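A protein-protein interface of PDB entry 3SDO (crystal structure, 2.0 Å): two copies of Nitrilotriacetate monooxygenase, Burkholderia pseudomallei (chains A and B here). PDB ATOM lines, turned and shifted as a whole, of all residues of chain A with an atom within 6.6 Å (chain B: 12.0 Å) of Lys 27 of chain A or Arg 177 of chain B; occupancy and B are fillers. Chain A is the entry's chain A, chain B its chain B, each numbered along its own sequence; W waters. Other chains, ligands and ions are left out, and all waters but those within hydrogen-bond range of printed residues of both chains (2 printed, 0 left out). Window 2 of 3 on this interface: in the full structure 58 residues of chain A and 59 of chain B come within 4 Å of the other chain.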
ATOM      1  N   ALA A  19     -29.659  23.291   3.615  1.00  0.00           N
ATOM      2  CA  ALA A  19     -30.230  22.564   2.478  1.00  0.00           C
ATOM      3  C   ALA A  19     -31.668  22.137   2.659  1.00  0.00           C
ATOM      4  O   ALA A  19     -32.410  22.053   1.677  1.00  0.00           O
ATOM      5  CB  ALA A  19     -29.366  21.336   2.129  1.00  0.00           C
ATOM      6  N   ASN A  24     -30.786  14.588   4.233  1.00  0.00           N
ATOM      7  CA  ASN A  24     -30.075  14.387   2.969  1.00  0.00           C
ATOM      8  C   ASN A  24     -30.431  15.396   1.865  1.00  0.00           C
ATOM      9  O   ASN A  24     -30.168  15.163   0.690  1.00  0.00           O
ATOM     10  CB  ASN A  24     -30.273  12.959   2.491  1.00  0.00           C
ATOM     11  CG  ASN A  24     -29.390  11.949   3.271  1.00  0.00           C
ATOM     12  OD1 ASN A  24     -28.573  12.334   4.130  1.00  0.00           O
ATOM     13  ND2 ASN A  24     -29.566  10.668   2.976  1.00  0.00           N
ATOM     14  N   ALA A  25     -30.958  16.546   2.272  1.00  0.00           N
ATOM     15  CA  ALA A  25     -31.391  17.573   1.330  1.00  0.00           C
ATOM     16  C   ALA A  25     -30.229  18.132   0.492  1.00  0.00           C
ATOM     17  O   ALA A  25     -30.455  18.655  -0.612  1.00  0.00           O
ATOM     18  CB  ALA A  25     -32.122  18.719   2.082  1.00  0.00           C
ATOM     19  N   TRP A  26     -28.999  18.023   0.998  1.00  0.00           N
ATOM     20  CA  TRP A  26     -27.810  18.495   0.250  1.00  0.00           C
ATOM     21  C   TRP A  26     -27.661  17.804  -1.112  1.00  0.00           C
ATOM     22  O   TRP A  26     -26.920  18.294  -1.982  1.00  0.00           O
ATOM     23  CB  TRP A  26     -26.509  18.290   1.039  1.00  0.00           C
ATOM     24  CG  TRP A  26     -26.094  16.857   1.238  1.00  0.00           C
ATOM     25  CD1 TRP A  26     -26.499  16.007   2.248  1.00  0.00           C
ATOM     26  CD2 TRP A  26     -25.180  16.103   0.432  1.00  0.00           C
ATOM     27  NE1 TRP A  26     -25.914  14.773   2.103  1.00  0.00           N
ATOM     28  CE2 TRP A  26     -25.093  14.800   1.000  1.00  0.00           C
ATOM     29  CE3 TRP A  26     -24.422  16.397  -0.703  1.00  0.00           C
ATOM     30  CZ2 TRP A  26     -24.279  13.803   0.468  1.00  0.00           C
ATOM     31  CZ3 TRP A  26     -23.624  15.384  -1.250  1.00  0.00           C
ATOM     32  CH2 TRP A  26     -23.552  14.110  -0.657  1.00  0.00           C
ATOM     33  N   LYS A  27     -28.292  16.638  -1.258  1.00  0.00           N
ATOM     34  CA  LYS A  27     -28.263  15.883  -2.512  1.00  0.00           C
ATOM     35  C   LYS A  27     -29.246  16.422  -3.559  1.00  0.00           C
ATOM     36  O   LYS A  27     -29.138  16.070  -4.736  1.00  0.00           O
ATOM     37  CB  LYS A  27     -28.611  14.401  -2.298  1.00  0.00           C
ATOM     38  CG  LYS A  27     -27.747  13.605  -1.334  1.00  0.00           C
ATOM     39  CD  LYS A  27     -28.138  12.108  -1.443  1.00  0.00           C
ATOM     40  CE  LYS A  27     -27.545  11.260  -0.347  1.00  0.00           C
ATOM     41  NZ  LYS A  27     -28.158   9.880  -0.223  1.00  0.00           N
ATOM     42  N   HIS A  28     -30.240  17.206  -3.142  1.00  0.00           N
ATOM     43  CA  HIS A  28     -31.279  17.647  -4.086  1.00  0.00           C
ATOM     44  C   HIS A  28     -30.769  18.755  -5.007  1.00  0.00           C
ATOM     45  O   HIS A  28     -30.174  19.720  -4.515  1.00  0.00           O
ATOM     46  CB  HIS A  28     -32.548  18.127  -3.366  1.00  0.00           C
ATOM     47  CG  HIS A  28     -33.739  18.118  -4.259  1.00  0.00           C
ATOM     48  ND1 HIS A  28     -34.124  19.221  -4.983  1.00  0.00           N
ATOM     49  CD2 HIS A  28     -34.558  17.108  -4.634  1.00  0.00           C
ATOM     50  CE1 HIS A  28     -35.164  18.899  -5.736  1.00  0.00           C
ATOM     51  NE2 HIS A  28     -35.439  17.618  -5.551  1.00  0.00           N
ATOM     52  N   PRO A  29     -31.018  18.632  -6.337  1.00  0.00           N
ATOM     53  CA  PRO A  29     -30.504  19.626  -7.293  1.00  0.00           C
ATOM     54  C   PRO A  29     -31.054  21.041  -7.165  1.00  0.00           C
ATOM     55  O   PRO A  29     -30.478  21.941  -7.731  1.00  0.00           O
ATOM     56  CB  PRO A  29     -30.873  19.050  -8.672  1.00  0.00           C
ATOM     57  CG  PRO A  29     -31.882  17.988  -8.424  1.00  0.00           C
ATOM     58  CD  PRO A  29     -31.690  17.503  -7.017  1.00  0.00           C
ATOM     59  N   SER A  30     -32.152  21.248  -6.442  1.00  0.00           N
ATOM     60  CA  SER A  30     -32.692  22.599  -6.273  1.00  0.00           C
ATOM     61  C   SER A  30     -31.920  23.462  -5.249  1.00  0.00           C
ATOM     62  O   SER A  30     -32.256  24.639  -5.060  1.00  0.00           O
ATOM     63  CB  SER A  30     -34.172  22.531  -5.877  1.00  0.00           C
ATOM     64  OG  SER A  30     -34.357  22.084  -4.518  1.00  0.00           O
ATOM     65  N   VAL A  31     -30.935  22.880  -4.565  1.00  0.00           N
ATOM     66  CA  VAL A  31     -30.069  23.630  -3.654  1.00  0.00           C
ATOM     67  C   VAL A  31     -28.603  23.396  -3.994  1.00  0.00           C
ATOM     68  O   VAL A  31     -28.270  22.378  -4.587  1.00  0.00           O
ATOM     69  CB  VAL A  31     -30.341  23.260  -2.152  1.00  0.00           C
ATOM     70  CG1 VAL A  31     -31.819  23.512  -1.783  1.00  0.00           C
ATOM     71  CG2 VAL A  31     -29.930  21.810  -1.868  1.00  0.00           C
ATOM     72  N   PRO A  32     -27.714  24.349  -3.639  1.00  0.00           N
ATOM     73  CA  PRO A  32     -26.280  24.039  -3.764  1.00  0.00           C
ATOM     74  C   PRO A  32     -25.866  22.965  -2.749  1.00  0.00           C
ATOM     75  O   PRO A  32     -26.402  22.931  -1.634  1.00  0.00           O
ATOM     76  CB  PRO A  32     -25.566  25.371  -3.434  1.00  0.00           C
ATOM     77  CG  PRO A  32     -26.569  26.269  -2.867  1.00  0.00           C
ATOM     78  CD  PRO A  32     -27.950  25.616  -2.921  1.00  0.00           C
ATOM     79  N   PRO A  33     -24.913  22.112  -3.112  1.00  0.00           N
ATOM     80  CA  PRO A  33     -24.490  21.035  -2.219  1.00  0.00           C
ATOM     81  C   PRO A  33     -23.993  21.538  -0.856  1.00  0.00           C
ATOM     82  O   PRO A  33     -24.226  20.884   0.165  1.00  0.00           O
ATOM     83  CB  PRO A  33     -23.317  20.363  -2.970  1.00  0.00           C
ATOM     84  CG  PRO A  33     -23.267  20.939  -4.299  1.00  0.00           C
ATOM     85  CD  PRO A  33     -24.167  22.131  -4.382  1.00  0.00           C
ATOM     86  N   ASP A  34     -23.324  22.692  -0.844  1.00  0.00           N
ATOM     87  CA  ASP A  34     -22.823  23.289   0.425  1.00  0.00           C
ATOM     88  C   ASP A  34     -23.818  24.280   1.047  1.00  0.00           C
ATOM     89  O   ASP A  34     -23.438  25.153   1.836  1.00  0.00           O
ATOM     90  CB  ASP A  34     -21.488  24.004   0.171  1.00  0.00           C
ATOM     91  CG  ASP A  34     -21.626  25.189  -0.768  1.00  0.00           C
ATOM     92  OD1 ASP A  34     -22.709  25.396  -1.331  1.00  0.00           O
ATOM     93  OD2 ASP A  34     -20.637  25.906  -0.958  1.00  0.00           O
ATOM     94  N   ASP A 293     -36.420   9.476  -1.775  1.00  0.00           N
ATOM     95  CA  ASP A 293     -35.232   8.859  -2.374  1.00  0.00           C
ATOM     96  C   ASP A 293     -33.915   9.601  -2.103  1.00  0.00           C
ATOM     97  O   ASP A 293     -32.866   9.180  -2.581  1.00  0.00           O
ATOM     98  CB  ASP A 293     -35.420   8.672  -3.876  1.00  0.00           C
ATOM     99  CG  ASP A 293     -36.504   7.651  -4.208  1.00  0.00           C
ATOM    100  OD1 ASP A 293     -36.938   6.885  -3.315  1.00  0.00           O
ATOM    101  OD2 ASP A 293     -36.931   7.626  -5.372  1.00  0.00           O
ATOM    102  N   LEU A 294     -33.976  10.685  -1.348  1.00  0.00           N
ATOM    103  CA  LEU A 294     -32.781  11.345  -0.823  1.00  0.00           C
ATOM    104  C   LEU A 294     -32.020  10.425   0.143  1.00  0.00           C
ATOM    105  O   LEU A 294     -30.800  10.519   0.266  1.00  0.00           O
ATOM    106  CB  LEU A 294     -33.158  12.640  -0.098  1.00  0.00           C
ATOM    107  CG  LEU A 294     -33.708  13.773  -0.982  1.00  0.00           C
ATOM    108  CD1 LEU A 294     -33.962  15.018  -0.156  1.00  0.00           C
ATOM    109  CD2 LEU A 294     -32.782  14.092  -2.130  1.00  0.00           C
ATOM    110  N   LEU A 295     -32.753   9.544   0.817  1.00  0.00           N
ATOM    111  CA  LEU A 295     -32.145   8.420   1.536  1.00  0.00           C
ATOM    112  C   LEU A 295     -31.924   7.281   0.538  1.00  0.00           C
ATOM    113  O   LEU A 295     -32.891   6.805  -0.075  1.00  0.00           O
ATOM    114  CB  LEU A 295     -33.097   7.960   2.650  1.00  0.00           C
ATOM    115  CG  LEU A 295     -32.521   7.215   3.838  1.00  0.00           C
ATOM    116  CD1 LEU A 295     -31.530   8.063   4.564  1.00  0.00           C
ATOM    117  CD2 LEU A 295     -33.642   6.813   4.781  1.00  0.00           C
ATOM    118  N   SER A 296     -30.682   6.823   0.380  1.00  0.00           N
ATOM    119  CA  SER A 296     -30.406   5.655  -0.472  1.00  0.00           C
ATOM    120  C   SER A 296     -30.957   4.374   0.199  1.00  0.00           C
ATOM    121  O   SER A 296     -31.199   4.362   1.401  1.00  0.00           O
ATOM    122  CB  SER A 296     -28.899   5.477  -0.707  1.00  0.00           C
ATOM    123  OG  SER A 296     -28.226   5.172   0.516  1.00  0.00           O
ATOM    124  N   GLU A 299     -28.907   3.355   3.218  1.00  0.00           N
ATOM    125  CA  GLU A 299     -29.088   4.190   4.402  1.00  0.00           C
ATOM    126  C   GLU A 299     -30.387   3.837   5.104  1.00  0.00           C
ATOM    127  O   GLU A 299     -30.431   3.766   6.340  1.00  0.00           O
ATOM    128  CB  GLU A 299     -29.082   5.669   4.050  1.00  0.00           C
ATOM    129  CG  GLU A 299     -27.706   6.268   3.795  1.00  0.00           C
ATOM    130  CD  GLU A 299     -27.828   7.701   3.301  1.00  0.00           C
ATOM    131  OE1 GLU A 299     -27.745   8.632   4.152  1.00  0.00           O
ATOM    132  OE2 GLU A 299     -28.083   7.884   2.087  1.00  0.00           O
ATOM    133  N   ALA B 172     -12.056  18.192   3.581  1.00  0.00           N
ATOM    134  CA  ALA B 172     -12.849  17.141   4.224  1.00  0.00           C
ATOM    135  C   ALA B 172     -14.267  17.035   3.657  1.00  0.00           C
ATOM    136  O   ALA B 172     -14.815  15.933   3.589  1.00  0.00           O
ATOM    137  CB  ALA B 172     -12.922  17.381   5.757  1.00  0.00           C
ATOM    138  N   LEU B 173     -14.868  18.171   3.289  1.00  0.00           N
ATOM    139  CA  LEU B 173     -16.274  18.210   2.855  1.00  0.00           C
ATOM    140  C   LEU B 173     -16.396  17.984   1.347  1.00  0.00           C
ATOM    141  O   LEU B 173     -16.595  18.915   0.553  1.00  0.00           O
ATOM    142  CB  LEU B 173     -16.975  19.498   3.302  1.00  0.00           C
ATOM    143  CG  LEU B 173     -17.141  19.607   4.815  1.00  0.00           C
ATOM    144  CD1 LEU B 173     -17.255  21.070   5.288  1.00  0.00           C
ATOM    145  CD2 LEU B 173     -18.369  18.777   5.323  1.00  0.00           C
ATOM    146  N   VAL B 174     -16.300  16.716   0.973  1.00  0.00           N
ATOM    147  CA  VAL B 174     -16.293  16.326  -0.412  1.00  0.00           C
ATOM    148  C   VAL B 174     -17.654  16.470  -1.071  1.00  0.00           C
ATOM    149  O   VAL B 174     -17.729  16.770  -2.259  1.00  0.00           O
ATOM    150  CB  VAL B 174     -15.766  14.873  -0.591  1.00  0.00           C
ATOM    151  CG1 VAL B 174     -14.295  14.803  -0.173  1.00  0.00           C
ATOM    152  CG2 VAL B 174     -16.629  13.863   0.191  1.00  0.00           C
ATOM    153  N   ARG B 175     -18.720  16.239  -0.309  1.00  0.00           N
ATOM    154  CA  ARG B 175     -20.091  16.399  -0.802  1.00  0.00           C
ATOM    155  C   ARG B 175     -20.264  15.825  -2.196  1.00  0.00           C
ATOM    156  O   ARG B 175     -20.666  16.525  -3.119  1.00  0.00           O
ATOM    157  CB  ARG B 175     -20.485  17.876  -0.802  1.00  0.00           C
ATOM    158  CG  ARG B 175     -20.279  18.550   0.525  1.00  0.00           C
ATOM    159  CD  ARG B 175     -21.097  19.799   0.559  1.00  0.00           C
ATOM    160  NE  ARG B 175     -20.814  20.689   1.662  1.00  0.00           N
ATOM    161  CZ  ARG B 175     -19.795  21.544   1.722  1.00  0.00           C
ATOM    162  NH1 ARG B 175     -18.892  21.615   0.745  1.00  0.00           N
ATOM    163  NH2 ARG B 175     -19.687  22.347   2.778  1.00  0.00           N
ATOM    164  N   ASP B 176     -19.956  14.544  -2.332  1.00  0.00           N
ATOM    165  CA  ASP B 176     -19.941  13.868  -3.613  1.00  0.00           C
ATOM    166  C   ASP B 176     -21.334  13.303  -3.865  1.00  0.00           C
ATOM    167  O   ASP B 176     -21.727  12.312  -3.242  1.00  0.00           O
ATOM    168  CB  ASP B 176     -18.873  12.771  -3.583  1.00  0.00           C
ATOM    169  CG  ASP B 176     -18.697  12.051  -4.923  1.00  0.00           C
ATOM    170  OD1 ASP B 176     -19.654  11.973  -5.731  1.00  0.00           O
ATOM    171  OD2 ASP B 176     -17.595  11.513  -5.135  1.00  0.00           O
ATOM    172  N   ARG B 177     -22.078  13.944  -4.777  1.00  0.00           N
ATOM    173  CA  ARG B 177     -23.450  13.536  -5.060  1.00  0.00           C
ATOM    174  C   ARG B 177     -23.496  12.244  -5.899  1.00  0.00           C
ATOM    175  O   ARG B 177     -24.485  11.535  -5.867  1.00  0.00           O
ATOM    176  CB  ARG B 177     -24.242  14.652  -5.764  1.00  0.00           C
ATOM    177  CG  ARG B 177     -24.611  15.846  -4.862  1.00  0.00           C
ATOM    178  CD  ARG B 177     -25.459  16.868  -5.606  1.00  0.00           C
ATOM    179  NE  ARG B 177     -26.070  17.876  -4.732  1.00  0.00           N
ATOM    180  CZ  ARG B 177     -26.579  19.036  -5.161  1.00  0.00           C
ATOM    181  NH1 ARG B 177     -26.542  19.363  -6.453  1.00  0.00           N
ATOM    182  NH2 ARG B 177     -27.097  19.900  -4.300  1.00  0.00           N
ATOM    183  N   ALA B 178     -22.425  11.952  -6.636  1.00  0.00           N
ATOM    184  CA  ALA B 178     -22.336  10.696  -7.392  1.00  0.00           C
ATOM    185  C   ALA B 178     -22.360   9.484  -6.455  1.00  0.00           C
ATOM    186  O   ALA B 178     -23.017   8.505  -6.747  1.00  0.00           O
ATOM    187  CB  ALA B 178     -21.075  10.673  -8.271  1.00  0.00           C
ATOM    188  N   THR B 179     -21.680   9.570  -5.309  1.00  0.00           N
ATOM    189  CA  THR B 179     -21.594   8.429  -4.374  1.00  0.00           C
ATOM    190  C   THR B 179     -22.450   8.577  -3.116  1.00  0.00           C
ATOM    191  O   THR B 179     -22.752   7.596  -2.450  1.00  0.00           O
ATOM    192  CB  THR B 179     -20.134   8.190  -3.943  1.00  0.00           C
ATOM    193  OG1 THR B 179     -19.663   9.318  -3.197  1.00  0.00           O
ATOM    194  CG2 THR B 179     -19.239   7.975  -5.189  1.00  0.00           C
ATOM    195  N   GLY B 180     -22.846   9.800  -2.784  1.00  0.00           N
ATOM    196  CA  GLY B 180     -23.548  10.056  -1.529  1.00  0.00           C
ATOM    197  C   GLY B 180     -22.636  10.274  -0.329  1.00  0.00           C
ATOM    198  O   GLY B 180     -23.120  10.375   0.792  1.00  0.00           O
ATOM    199  N   ARG B 181     -21.321  10.346  -0.544  1.00  0.00           N
ATOM    200  CA  ARG B 181     -20.392  10.581   0.562  1.00  0.00           C
ATOM    201  C   ARG B 181     -20.352  12.095   0.834  1.00  0.00           C
ATOM    202  O   ARG B 181     -19.941  12.879  -0.032  1.00  0.00           O
ATOM    203  CB  ARG B 181     -18.984  10.027   0.242  1.00  0.00           C
ATOM    204  CG  ARG B 181     -17.955  10.183   1.389  1.00  0.00           C
ATOM    205  CD  ARG B 181     -16.648   9.431   1.109  1.00  0.00           C
ATOM    206  NE  ARG B 181     -15.994   9.993  -0.077  1.00  0.00           N
ATOM    207  CZ  ARG B 181     -14.732  10.409  -0.157  1.00  0.00           C
ATOM    208  NH1 ARG B 181     -13.886  10.298   0.866  1.00  0.00           N
ATOM    209  NH2 ARG B 181     -14.310  10.927  -1.298  1.00  0.00           N
ATOM    210  N   PHE B 182     -20.803  12.500   2.023  1.00  0.00           N
ATOM    211  CA  PHE B 182     -20.859  13.912   2.364  1.00  0.00           C
ATOM    212  C   PHE B 182     -19.500  14.450   2.792  1.00  0.00           C
ATOM    213  O   PHE B 182     -19.114  15.580   2.441  1.00  0.00           O
ATOM    214  CB  PHE B 182     -21.873  14.160   3.483  1.00  0.00           C
ATOM    215  CG  PHE B 182     -22.025  15.624   3.846  1.00  0.00           C
ATOM    216  CD1 PHE B 182     -21.567  16.109   5.061  1.00  0.00           C
ATOM    217  CD2 PHE B 182     -22.604  16.517   2.954  1.00  0.00           C
ATOM    218  CE1 PHE B 182     -21.711  17.458   5.399  1.00  0.00           C
ATOM    219  CE2 PHE B 182     -22.766  17.866   3.294  1.00  0.00           C
ATOM    220  CZ  PHE B 182     -22.307  18.330   4.496  1.00  0.00           C
ATOM    221  N   PHE B 183     -18.785  13.654   3.584  1.00  0.00           N
ATOM    222  CA  PHE B 183     -17.481  14.055   4.078  1.00  0.00           C
ATOM    223  C   PHE B 183     -16.561  12.855   4.290  1.00  0.00           C
ATOM    224  O   PHE B 183     -17.028  11.719   4.379  1.00  0.00           O
ATOM    225  CB  PHE B 183     -17.634  14.839   5.383  1.00  0.00           C
ATOM    226  CG  PHE B 183     -17.888  13.980   6.605  1.00  0.00           C
ATOM    227  CD1 PHE B 183     -19.098  13.304   6.764  1.00  0.00           C
ATOM    228  CD2 PHE B 183     -16.925  13.877   7.619  1.00  0.00           C
ATOM    229  CE1 PHE B 183     -19.349  12.534   7.896  1.00  0.00           C
ATOM    230  CE2 PHE B 183     -17.175  13.112   8.757  1.00  0.00           C
ATOM    231  CZ  PHE B 183     -18.386  12.446   8.897  1.00  0.00           C
ATOM    232  N   ASP B 184     -15.256  13.125   4.373  1.00  0.00           N
ATOM    233  CA  ASP B 184     -14.267  12.089   4.682  1.00  0.00           C
ATOM    234  C   ASP B 184     -14.080  12.034   6.202  1.00  0.00           C
ATOM    235  O   ASP B 184     -13.521  12.981   6.795  1.00  0.00           O
ATOM    236  CB  ASP B 184     -12.929  12.415   4.022  1.00  0.00           C
ATOM    237  CG  ASP B 184     -11.877  11.331   4.257  1.00  0.00           C
ATOM    238  OD1 ASP B 184     -12.005  10.540   5.228  1.00  0.00           O
ATOM    239  OD2 ASP B 184     -10.940  11.267   3.454  1.00  0.00           O
HETATM  240  O   HOH W   1     -27.441  21.835  -7.248  1.00  0.00           O
HETATM  241  O   HOH W   2     -25.607  10.209   1.715  1.00  0.00           O
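Water W2 lies within hydrogen-bond range of O of Gly 180 of chain B, NZ of Lys 27 of chain A and OE2 of Glu 299 of chain A. Water W1 lies within hydrogen-bond range of the guanidinium group of Arg 177 of chain B, the backbone carbonyl oxygen of Val 31 of chain A and the backbone carbonyl oxygen of Pro 29 of chain A.
Printed residues of chain B that touch a printed residue of chain A: Arg 175, Asp 176, Arg 177, Gly 180, Arg 181 and Phe 182. Hydrophobic or aromatic side chains of chain B within 4 Å of the printed part of chain A: Phe 182. Hydrophobic or aromatic side chains of chain A that line the printed part of chain B: Trp 26 and Pro 33. Among the printed residues, no Asp or Glu carboxylate lies within 4 Å of a Lys or Arg side-chain nitrogen of the other chain.
Lys 27 of chain A touches just one residue of chain B: Arg 177 (3.6 Å). Of chain A, only Trp 26 (2.8 Å), Lys 27 (3.6 Å), His 28 (3.1 Å), Val 31 (2.8 Å), Pro 32 (3.6 Å) and Pro 33 (3.3 Å) come within 4 Å of Arg 177 of chain B. No residue of chain B comes within 4 Å of Asn 24 of chain A. No residue of chain B comes within 4 Å of Ala 25 of chain A. Of chain B, only Arg 175, Asp 176, Arg 177, Gly 180, Arg 181 and Phe 182 come within 4 Å of Trp 26 of chain A. His 28 of chain A touches just one residue of chain B: Arg 177 (3.1 Å). No residue of chain B comes within 4 Å of Pro 29 of chain A. No residue of chain B comes within 4 Å of Ser 30 of chain A. Printed residues of chain B within 4 Å of Pro 32 of chain A: Arg 177 (3.6 Å). Pro 33 of chain A touches just these residues of chain B: Arg 175 (3.3 Å) and Arg 177 (3.3 Å). Ser 296 of chain A touches none of the printed residues of chain B. Printed residues of chain A within 4 Å of Arg 175 of chain B: Trp 26, Pro 33 and Asp 34. Of the printed residues of chain A, Phe 182 of chain B touches Trp 26. Of the printed residues of chain B, Asp 34 of chain A touches Arg 175 (3.4 Å). The nearest residue of chain B that does not touch Lys 27 of chain A is Gly 180 of chain B (4.3 Å). The nearest residue of chain A that does not touch Arg 177 of chain B is Pro 29 of chain A (4.1 Å). The nearest printed residue of chain A that does not touch Phe 182 of chain B is Pro 33 of chain A (4.6 Å).
No position is printed for both chains.
The side-chain carboxylate (OD1) of Asp 176 of chain B is in hydrogen-bond range of the backbone NH (N) of Ala 178 of chain B, 2.9 Å away. O of Leu 294 of chain A sits at hydrogen-bond distance from NZ of Lys 27 of chain A. OG1 of Thr 179 of chain B sits at hydrogen-bond distance from N of Arg 181 of chain B (3.3 Å). NZ of Lys 27 of chain A is in salt-bridge range of OE2 of Glu 299 of chain A. N of Arg 175 of chain B sits at hydrogen-bond distance from O of Phe 182 of chain B (2.9 Å). The side-chain carboxylate of Asp 176 of chain B is in hydrogen-bond range of the backbone NH of Thr 179 of chain B (3.2 Å).
N of Pro 33 of chain A sits close to NH2 of Arg 177 of chain B, 3.3 Å away. The backbone carbonyl oxygen (O) of Val 31 of chain A sits at hydrogen-bond distance from the guanidinium group (NH2) of Arg 177 of chain B (2.8 Å). The backbone carbonyl oxygen of Trp 26 of chain A lies within hydrogen-bond range of the guanidinium group of Arg 177 of chain B, at 2.8 Å. NH2 of Arg 177 of chain B is in hydrogen-bond range of O of His 28 of chain A, 3.1 Å away.
Among the printed residues, pairs that only touch across the chains: Trp 26 of chain A with Arg 175 of chain B (3.5 Å), Trp 26 of chain A with Asp 176 of chain B (3.6 Å), Trp 26 of chain A with Gly 180 of chain B (3.6 Å), Trp 26 of chain A with Arg 181 of chain B (3.9 Å), Trp 26 of chain A with Phe 182 of chain B (3.6 Å), Lys 27 of chain A with Arg 177 of chain B (3.6 Å), Pro 32 of chain A with Arg 177 of chain B (3.6 Å), Pro 33 of chain A with Arg 175 of chain B (3.3 Å) and Asp 34 of chain A with Arg 175 of chain B (3.4 Å).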
